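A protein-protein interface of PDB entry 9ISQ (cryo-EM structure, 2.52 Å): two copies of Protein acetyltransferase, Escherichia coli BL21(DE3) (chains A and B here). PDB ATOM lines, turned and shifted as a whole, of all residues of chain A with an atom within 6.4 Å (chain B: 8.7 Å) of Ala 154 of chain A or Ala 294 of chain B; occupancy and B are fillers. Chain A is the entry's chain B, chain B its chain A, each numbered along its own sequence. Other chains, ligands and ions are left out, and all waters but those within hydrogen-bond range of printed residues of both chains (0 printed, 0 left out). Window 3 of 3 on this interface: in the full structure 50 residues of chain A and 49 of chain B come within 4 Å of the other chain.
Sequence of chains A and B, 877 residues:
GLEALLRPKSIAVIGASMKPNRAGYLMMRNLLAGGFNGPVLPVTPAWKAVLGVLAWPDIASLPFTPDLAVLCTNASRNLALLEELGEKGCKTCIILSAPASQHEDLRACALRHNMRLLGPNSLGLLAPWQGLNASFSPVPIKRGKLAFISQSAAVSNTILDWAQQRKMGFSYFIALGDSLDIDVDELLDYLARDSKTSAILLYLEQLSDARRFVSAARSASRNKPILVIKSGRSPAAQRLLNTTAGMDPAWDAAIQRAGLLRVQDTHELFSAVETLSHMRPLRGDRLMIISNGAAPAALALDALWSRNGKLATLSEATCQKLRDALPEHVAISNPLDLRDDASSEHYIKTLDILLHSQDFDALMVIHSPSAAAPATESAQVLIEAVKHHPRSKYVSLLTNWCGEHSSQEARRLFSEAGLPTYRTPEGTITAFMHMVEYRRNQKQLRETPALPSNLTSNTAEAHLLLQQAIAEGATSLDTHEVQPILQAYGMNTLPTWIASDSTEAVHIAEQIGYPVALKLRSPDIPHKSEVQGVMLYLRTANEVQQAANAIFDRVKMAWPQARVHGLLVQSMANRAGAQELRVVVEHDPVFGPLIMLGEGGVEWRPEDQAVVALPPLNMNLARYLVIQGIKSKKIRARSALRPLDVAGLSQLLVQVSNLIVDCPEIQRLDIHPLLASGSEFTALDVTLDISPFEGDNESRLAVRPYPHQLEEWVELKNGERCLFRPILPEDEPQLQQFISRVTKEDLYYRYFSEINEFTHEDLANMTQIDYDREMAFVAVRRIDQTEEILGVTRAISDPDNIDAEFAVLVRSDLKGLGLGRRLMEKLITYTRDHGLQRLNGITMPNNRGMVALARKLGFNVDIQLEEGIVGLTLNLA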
ATOM      1  N   ASN A 121     -13.520  -7.339  -3.256  1.00  0.00           N
ATOM      2  CA  ASN A 121     -12.165  -7.498  -2.739  1.00  0.00           C
ATOM      3  C   ASN A 121     -11.253  -8.098  -3.804  1.00  0.00           C
ATOM      4  O   ASN A 121     -10.421  -8.962  -3.525  1.00  0.00           O
ATOM      5  CB  ASN A 121     -12.156  -8.344  -1.464  1.00  0.00           C
ATOM      6  CG  ASN A 121     -13.199  -7.891  -0.458  1.00  0.00           C
ATOM      7  OD1 ASN A 121     -14.223  -8.543  -0.267  1.00  0.00           O
ATOM      8  ND2 ASN A 121     -12.939  -6.766   0.193  1.00  0.00           N
ATOM      9  N   SER A 152      -7.077 -14.524  -3.571  1.00  0.00           N
ATOM     10  CA  SER A 152      -7.157 -13.505  -2.534  1.00  0.00           C
ATOM     11  C   SER A 152      -6.469 -12.220  -2.979  1.00  0.00           C
ATOM     12  O   SER A 152      -5.470 -12.246  -3.702  1.00  0.00           O
ATOM     13  CB  SER A 152      -6.528 -14.002  -1.229  1.00  0.00           C
ATOM     14  OG  SER A 152      -6.857 -13.153  -0.143  1.00  0.00           O
ATOM     15  N   ALA A 153      -7.019 -11.088  -2.532  1.00  0.00           N
ATOM     16  CA  ALA A 153      -6.425  -9.796  -2.862  1.00  0.00           C
ATOM     17  C   ALA A 153      -5.031  -9.665  -2.268  1.00  0.00           C
ATOM     18  O   ALA A 153      -4.120  -9.142  -2.917  1.00  0.00           O
ATOM     19  CB  ALA A 153      -7.320  -8.661  -2.370  1.00  0.00           C
ATOM     20  N   ALA A 154      -4.845 -10.119  -1.028  1.00  0.00           N
ATOM     21  CA  ALA A 154      -3.497 -10.191  -0.477  1.00  0.00           C
ATOM     22  C   ALA A 154      -2.637 -11.131  -1.306  1.00  0.00           C
ATOM     23  O   ALA A 154      -1.511 -10.790  -1.689  1.00  0.00           O
ATOM     24  CB  ALA A 154      -3.549 -10.650   0.980  1.00  0.00           C
ATOM     25  N   VAL A 155      -3.174 -12.311  -1.623  1.00  0.00           N
ATOM     26  CA  VAL A 155      -2.467 -13.248  -2.487  1.00  0.00           C
ATOM     27  C   VAL A 155      -2.245 -12.638  -3.859  1.00  0.00           C
ATOM     28  O   VAL A 155      -1.166 -12.771  -4.443  1.00  0.00           O
ATOM     29  CB  VAL A 155      -3.245 -14.570  -2.597  1.00  0.00           C
ATOM     30  CG1 VAL A 155      -2.611 -15.463  -3.644  1.00  0.00           C
ATOM     31  CG2 VAL A 155      -3.293 -15.281  -1.263  1.00  0.00           C
ATOM     32  N   SER A 156      -3.268 -11.987  -4.410  1.00  0.00           N
ATOM     33  CA  SER A 156      -3.149 -11.438  -5.755  1.00  0.00           C
ATOM     34  C   SER A 156      -2.056 -10.381  -5.817  1.00  0.00           C
ATOM     35  O   SER A 156      -1.243 -10.367  -6.745  1.00  0.00           O
ATOM     36  CB  SER A 156      -4.488 -10.859  -6.203  1.00  0.00           C
ATOM     37  OG  SER A 156      -5.451 -11.884  -6.368  1.00  0.00           O
ATOM     38  N   ASN A 157      -2.022  -9.484  -4.828  1.00  0.00           N
ATOM     39  CA  ASN A 157      -1.002  -8.443  -4.810  1.00  0.00           C
ATOM     40  C   ASN A 157       0.379  -9.031  -4.575  1.00  0.00           C
ATOM     41  O   ASN A 157       1.342  -8.649  -5.248  1.00  0.00           O
ATOM     42  CB  ASN A 157      -1.320  -7.403  -3.739  1.00  0.00           C
ATOM     43  CG  ASN A 157      -1.194  -5.990  -4.256  1.00  0.00           C
ATOM     44  OD1 ASN A 157      -0.298  -5.685  -5.043  1.00  0.00           O
ATOM     45  ND2 ASN A 157      -2.092  -5.117  -3.820  1.00  0.00           N
ATOM     46  N   THR A 158       0.497  -9.972  -3.640  1.00  0.00           N
ATOM     47  CA  THR A 158       1.778 -10.622  -3.414  1.00  0.00           C
ATOM     48  C   THR A 158       2.280 -11.281  -4.690  1.00  0.00           C
ATOM     49  O   THR A 158       3.452 -11.146  -5.059  1.00  0.00           O
ATOM     50  CB  THR A 158       1.636 -11.652  -2.298  1.00  0.00           C
ATOM     51  OG1 THR A 158       1.118 -11.011  -1.126  1.00  0.00           O
ATOM     52  CG2 THR A 158       2.982 -12.291  -1.980  1.00  0.00           C
ATOM     53  N   ILE A 159       1.396 -11.989  -5.391  1.00  0.00           N
ATOM     54  CA  ILE A 159       1.816 -12.728  -6.570  1.00  0.00           C
ATOM     55  C   ILE A 159       2.150 -11.780  -7.713  1.00  0.00           C
ATOM     56  O   ILE A 159       3.142 -11.979  -8.413  1.00  0.00           O
ATOM     57  CB  ILE A 159       0.737 -13.745  -6.980  1.00  0.00           C
ATOM     58  CG1 ILE A 159       0.603 -14.838  -5.913  1.00  0.00           C
ATOM     59  CG2 ILE A 159       1.082 -14.347  -8.331  1.00  0.00           C
ATOM     60  CD1 ILE A 159       1.725 -15.855  -5.911  1.00  0.00           C
ATOM     61  N   LEU A 240      -5.332 -18.528  10.075  1.00  0.00           N
ATOM     62  CA  LEU A 240      -5.125 -17.176   9.565  1.00  0.00           C
ATOM     63  C   LEU A 240      -5.871 -16.937   8.259  1.00  0.00           C
ATOM     64  O   LEU A 240      -6.127 -15.782   7.903  1.00  0.00           O
ATOM     65  CB  LEU A 240      -3.636 -16.901   9.369  1.00  0.00           C
ATOM     66  CG  LEU A 240      -3.307 -15.487   8.888  1.00  0.00           C
ATOM     67  CD1 LEU A 240      -2.274 -14.844   9.794  1.00  0.00           C
ATOM     68  CD2 LEU A 240      -2.817 -15.509   7.454  1.00  0.00           C
ATOM     69  N   LEU A 241      -6.226 -17.998   7.537  1.00  0.00           N
ATOM     70  CA  LEU A 241      -6.967 -17.878   6.291  1.00  0.00           C
ATOM     71  C   LEU A 241      -8.418 -18.329   6.412  1.00  0.00           C
ATOM     72  O   LEU A 241      -9.187 -18.138   5.465  1.00  0.00           O
ATOM     73  CB  LEU A 241      -6.276 -18.684   5.184  1.00  0.00           C
ATOM     74  CG  LEU A 241      -4.881 -18.220   4.749  1.00  0.00           C
ATOM     75  CD1 LEU A 241      -4.296 -19.191   3.749  1.00  0.00           C
ATOM     76  CD2 LEU A 241      -4.913 -16.824   4.163  1.00  0.00           C
ATOM     77  N   ILE B 289       6.507 -12.535  13.788  1.00  0.00           N
ATOM     78  CA  ILE B 289       6.435 -12.181  12.373  1.00  0.00           C
ATOM     79  C   ILE B 289       5.530 -10.968  12.206  1.00  0.00           C
ATOM     80  O   ILE B 289       4.518 -10.839  12.900  1.00  0.00           O
ATOM     81  CB  ILE B 289       5.929 -13.357  11.506  1.00  0.00           C
ATOM     82  CG1 ILE B 289       6.886 -14.547  11.578  1.00  0.00           C
ATOM     83  CG2 ILE B 289       5.770 -12.938  10.054  1.00  0.00           C
ATOM     84  CD1 ILE B 289       6.365 -15.706  12.381  1.00  0.00           C
ATOM     85  N   SER B 291       4.064  -8.440   8.735  1.00  0.00           N
ATOM     86  CA  SER B 291       4.022  -8.339   7.283  1.00  0.00           C
ATOM     87  C   SER B 291       2.801  -7.528   6.871  1.00  0.00           C
ATOM     88  O   SER B 291       1.920  -7.237   7.680  1.00  0.00           O
ATOM     89  CB  SER B 291       3.992  -9.725   6.637  1.00  0.00           C
ATOM     90  OG  SER B 291       2.771 -10.388   6.912  1.00  0.00           O
ATOM     91  N   ASN B 292       2.760  -7.172   5.585  1.00  0.00           N
ATOM     92  CA  ASN B 292       1.648  -6.439   4.992  1.00  0.00           C
ATOM     93  C   ASN B 292       0.854  -7.302   4.012  1.00  0.00           C
ATOM     94  O   ASN B 292       0.388  -6.812   2.983  1.00  0.00           O
ATOM     95  CB  ASN B 292       2.146  -5.174   4.294  1.00  0.00           C
ATOM     96  CG  ASN B 292       3.072  -5.467   3.125  1.00  0.00           C
ATOM     97  OD1 ASN B 292       3.298  -6.622   2.767  1.00  0.00           O
ATOM     98  ND2 ASN B 292       3.613  -4.418   2.523  1.00  0.00           N
ATOM     99  N   GLY B 293       0.702  -8.587   4.315  1.00  0.00           N
ATOM    100  CA  GLY B 293      -0.053  -9.492   3.469  1.00  0.00           C
ATOM    101  C   GLY B 293      -0.213 -10.859   4.100  1.00  0.00           C
ATOM    102  O   GLY B 293       0.636 -11.281   4.890  1.00  0.00           O
ATOM    103  N   ALA B 294      -1.293 -11.565   3.763  1.00  0.00           N
ATOM    104  CA  ALA B 294      -1.588 -12.836   4.418  1.00  0.00           C
ATOM    105  C   ALA B 294      -0.766 -13.982   3.841  1.00  0.00           C
ATOM    106  O   ALA B 294      -0.184 -14.770   4.591  1.00  0.00           O
ATOM    107  CB  ALA B 294      -3.080 -13.147   4.305  1.00  0.00           C
ATOM    108  N   ALA B 295      -0.707 -14.091   2.516  1.00  0.00           N
ATOM    109  CA  ALA B 295      -0.090 -15.265   1.903  1.00  0.00           C
ATOM    110  C   ALA B 295       1.360 -15.450   2.313  1.00  0.00           C
ATOM    111  O   ALA B 295       1.719 -16.559   2.746  1.00  0.00           O
ATOM    112  CB  ALA B 295      -0.218 -15.176   0.383  1.00  0.00           C
ATOM    113  N   PRO B 296       2.234 -14.441   2.231  1.00  0.00           N
ATOM    114  CA  PRO B 296       3.643 -14.688   2.576  1.00  0.00           C
ATOM    115  C   PRO B 296       3.810 -15.318   3.942  1.00  0.00           C
ATOM    116  O   PRO B 296       4.417 -16.391   4.055  1.00  0.00           O
ATOM    117  CB  PRO B 296       4.271 -13.289   2.510  1.00  0.00           C
ATOM    118  CG  PRO B 296       3.349 -12.484   1.689  1.00  0.00           C
ATOM    119  CD  PRO B 296       1.986 -13.024   1.924  1.00  0.00           C
ATOM    120  N   ALA B 297       3.251 -14.698   4.981  1.00  0.00           N
ATOM    121  CA  ALA B 297       3.340 -15.273   6.317  1.00  0.00           C
ATOM    122  C   ALA B 297       2.830 -16.706   6.330  1.00  0.00           C
ATOM    123  O   ALA B 297       3.454 -17.587   6.931  1.00  0.00           O
ATOM    124  CB  ALA B 297       2.557 -14.415   7.307  1.00  0.00           C
ATOM    125  N   ALA B 298       1.711 -16.969   5.651  1.00  0.00           N
ATOM    126  CA  ALA B 298       1.203 -18.333   5.593  1.00  0.00           C
ATOM    127  C   ALA B 298       2.250 -19.275   5.020  1.00  0.00           C
ATOM    128  O   ALA B 298       2.534 -20.328   5.602  1.00  0.00           O
ATOM    129  CB  ALA B 298      -0.076 -18.381   4.763  1.00  0.00           C
ATOM    130  N   LEU B 299       2.870 -18.889   3.902  1.00  0.00           N
ATOM    131  CA  LEU B 299       3.906 -19.727   3.312  1.00  0.00           C
ATOM    132  C   LEU B 299       5.031 -19.973   4.304  1.00  0.00           C
ATOM    133  O   LEU B 299       5.642 -21.047   4.307  1.00  0.00           O
ATOM    134  CB  LEU B 299       4.447 -19.080   2.041  1.00  0.00           C
ATOM    135  CG  LEU B 299       3.457 -18.981   0.882  1.00  0.00           C
ATOM    136  CD1 LEU B 299       3.877 -17.889  -0.086  1.00  0.00           C
ATOM    137  CD2 LEU B 299       3.334 -20.311   0.166  1.00  0.00           C
ATOM    138  N   ALA B 300       5.320 -18.988   5.155  1.00  0.00           N
ATOM    139  CA  ALA B 300       6.334 -19.190   6.181  1.00  0.00           C
ATOM    140  C   ALA B 300       5.861 -20.202   7.215  1.00  0.00           C
ATOM    141  O   ALA B 300       6.594 -21.132   7.568  1.00  0.00           O
ATOM    142  CB  ALA B 300       6.681 -17.858   6.840  1.00  0.00           C
ATOM    143  N   LEU B 301       4.616 -20.063   7.677  1.00  0.00           N
ATOM    144  CA  LEU B 301       4.142 -20.895   8.776  1.00  0.00           C
ATOM    145  C   LEU B 301       4.267 -22.370   8.436  1.00  0.00           C
ATOM    146  O   LEU B 301       4.812 -23.158   9.220  1.00  0.00           O
ATOM    147  CB  LEU B 301       2.695 -20.541   9.110  1.00  0.00           C
ATOM    148  CG  LEU B 301       2.468 -19.195   9.795  1.00  0.00           C
ATOM    149  CD1 LEU B 301       1.004 -19.028  10.136  1.00  0.00           C
ATOM    150  CD2 LEU B 301       3.316 -19.067  11.047  1.00  0.00           C
ATOM    151  N   LEU B 336       1.389 -12.838  14.151  1.00  0.00           N
ATOM    152  CA  LEU B 336       1.642 -12.318  12.811  1.00  0.00           C
ATOM    153  C   LEU B 336       0.756 -11.094  12.610  1.00  0.00           C
ATOM    154  O   LEU B 336      -0.415 -11.219  12.244  1.00  0.00           O
ATOM    155  CB  LEU B 336       1.381 -13.375  11.748  1.00  0.00           C
ATOM    156  CG  LEU B 336       1.907 -14.767  12.082  1.00  0.00           C
ATOM    157  CD1 LEU B 336       0.791 -15.646  12.600  1.00  0.00           C
ATOM    158  CD2 LEU B 336       2.551 -15.384  10.859  1.00  0.00           C
ATOM    159  N   ASP B 337       1.313  -9.913  12.858  1.00  0.00           N
ATOM    160  CA  ASP B 337       0.613  -8.686  12.517  1.00  0.00           C
ATOM    161  C   ASP B 337       0.338  -8.660  11.021  1.00  0.00           C
ATOM    162  O   ASP B 337       1.180  -9.059  10.212  1.00  0.00           O
ATOM    163  CB  ASP B 337       1.437  -7.468  12.932  1.00  0.00           C
ATOM    164  CG  ASP B 337       0.871  -6.768  14.152  1.00  0.00           C
ATOM    165  OD1 ASP B 337      -0.354  -6.837  14.371  1.00  0.00           O
ATOM    166  OD2 ASP B 337       1.656  -6.149  14.896  1.00  0.00           O
ATOM    167  N   LEU B 338      -0.846  -8.192  10.651  1.00  0.00           N
ATOM    168  CA  LEU B 338      -1.310  -8.272   9.278  1.00  0.00           C
ATOM    169  C   LEU B 338      -1.887  -6.934   8.850  1.00  0.00           C
ATOM    170  O   LEU B 338      -2.679  -6.326   9.575  1.00  0.00           O
ATOM    171  CB  LEU B 338      -2.361  -9.376   9.126  1.00  0.00           C
ATOM    172  CG  LEU B 338      -2.584  -9.977   7.738  1.00  0.00           C
ATOM    173  CD1 LEU B 338      -3.182  -8.988   6.755  1.00  0.00           C
ATOM    174  CD2 LEU B 338      -1.278 -10.530   7.207  1.00  0.00           C
ATOM    175  N   ARG B 339      -1.476  -6.477   7.671  1.00  0.00           N
ATOM    176  CA  ARG B 339      -1.988  -5.257   7.073  1.00  0.00           C
ATOM    177  C   ARG B 339      -2.131  -5.488   5.577  1.00  0.00           C
ATOM    178  O   ARG B 339      -1.676  -6.499   5.040  1.00  0.00           O
ATOM    179  CB  ARG B 339      -1.065  -4.068   7.355  1.00  0.00           C
ATOM    180  CG  ARG B 339      -0.819  -3.803   8.832  1.00  0.00           C
ATOM    181  CD  ARG B 339       0.277  -4.694   9.399  1.00  0.00           C
ATOM    182  NE  ARG B 339       1.189  -3.974  10.281  1.00  0.00           N
ATOM    183  CZ  ARG B 339       2.316  -3.396   9.890  1.00  0.00           C
ATOM    184  NH1 ARG B 339       2.704  -3.415   8.626  1.00  0.00           N
ATOM    185  NH2 ARG B 339       3.078  -2.787  10.793  1.00  0.00           N
ATOM    186  N   ASP B 340      -2.779  -4.562   4.907  1.00  0.00           N
ATOM    187  CA  ASP B 340      -2.960  -4.657   3.461  1.00  0.00           C
ATOM    188  C   ASP B 340      -2.457  -3.429   2.719  1.00  0.00           C
ATOM    189  O   ASP B 340      -1.858  -3.566   1.652  1.00  0.00           O
ATOM    190  CB  ASP B 340      -4.448  -4.878   3.144  1.00  0.00           C
ATOM    191  CG  ASP B 340      -4.932  -6.265   3.533  1.00  0.00           C
ATOM    192  OD1 ASP B 340      -4.081  -7.149   3.779  1.00  0.00           O
ATOM    193  OD2 ASP B 340      -6.163  -6.469   3.596  1.00  0.00           O
ATOM    194  N   ILE B 366       8.391  -8.816   6.785  1.00  0.00           N
ATOM    195  CA  ILE B 366       8.152  -9.133   5.383  1.00  0.00           C
ATOM    196  C   ILE B 366       7.542  -7.917   4.709  1.00  0.00           C
ATOM    197  O   ILE B 366       6.694  -7.235   5.293  1.00  0.00           O
ATOM    198  CB  ILE B 366       7.229 -10.360   5.225  1.00  0.00           C
ATOM    199  CG1 ILE B 366       7.711 -11.517   6.105  1.00  0.00           C
ATOM    200  CG2 ILE B 366       7.161 -10.800   3.775  1.00  0.00           C
ATOM    201  CD1 ILE B 366       6.860 -12.752   6.002  1.00  0.00           C
ATOM    202  N   SER B 368       5.929  -6.708   0.835  1.00  0.00           N
ATOM    203  CA  SER B 368       5.542  -6.859  -0.561  1.00  0.00           C
ATOM    204  C   SER B 368       5.362  -5.471  -1.156  1.00  0.00           C
ATOM    205  O   SER B 368       4.500  -4.721  -0.674  1.00  0.00           O
ATOM    206  CB  SER B 368       4.251  -7.662  -0.693  1.00  0.00           C
ATOM    207  OG  SER B 368       4.452  -9.028  -0.385  1.00  0.00           O
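Along chain B the printed residues that touch a printed residue of chain A span positions 294 to 368.
Of the 11 printed residues of chain A, 4 touch a printed residue of chain B.
Among the printed residues, no Asp or Glu carboxylate lies within 4 Å of a Lys or Arg side-chain nitrogen of the other chain.
No residue of chain B comes within 4 Å of Ala 153 of chain A.
Ala 154 of chain A touches just one residue of chain B: Ala 294 (3.7 Å).
Of the printed residues of chain B, Val 155 of chain A touches Ala 295.
Of the printed residues of chain B, Thr 158 of chain A touches Pro 296 (3.7 Å) and Ser 368 (3.9 Å).
Of chain A, only Ala 154 (3.7 Å) and Leu 240 (3.9 Å) come within 4 Å of Ala 294 of chain B.
Printed residues of chain A within 4 Å of Ala 295 of chain B: Val 155.
Of the printed residues of chain A, Pro 296 of chain B touches Thr 158 (3.7 Å).
Ala 297 of chain B touches none of the printed residues of chain A.
Ala 298 of chain B touches none of the printed residues of chain A.
The nearest residue of chain B that does not touch Ala 154 of chain A is Gly 293 of chain B (4.4 Å).
Among the printed residues, pairs that only touch across the chains: Val 155 of chain A with Ala 295 of chain B (3.5 Å), Thr 158 of chain A with Pro 296 of chain B (3.7 Å), Ala 154 of chain A with Ala 294 of chain B (3.7 Å), Thr 158 of chain A with Ser 368 of chain B (3.9 Å) and Leu 240 of chain A with Ala 294 of chain B (3.9 Å).
The side-chain amide oxygen (OD1) of Asn 292 of chain B lies within hydrogen-bond range of the backbone NH (N) of Ser 368 of chain B, at 3.3 Å.
OG1 of Thr 158 of chain A is in hydrogen-bond range of O of Ala 154 of chain A (2.7 Å).
No position is printed for both chains.
Of the 5 pairs that touch across the chains among the printed residues, none has its exchanged pair printed and touching as well.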
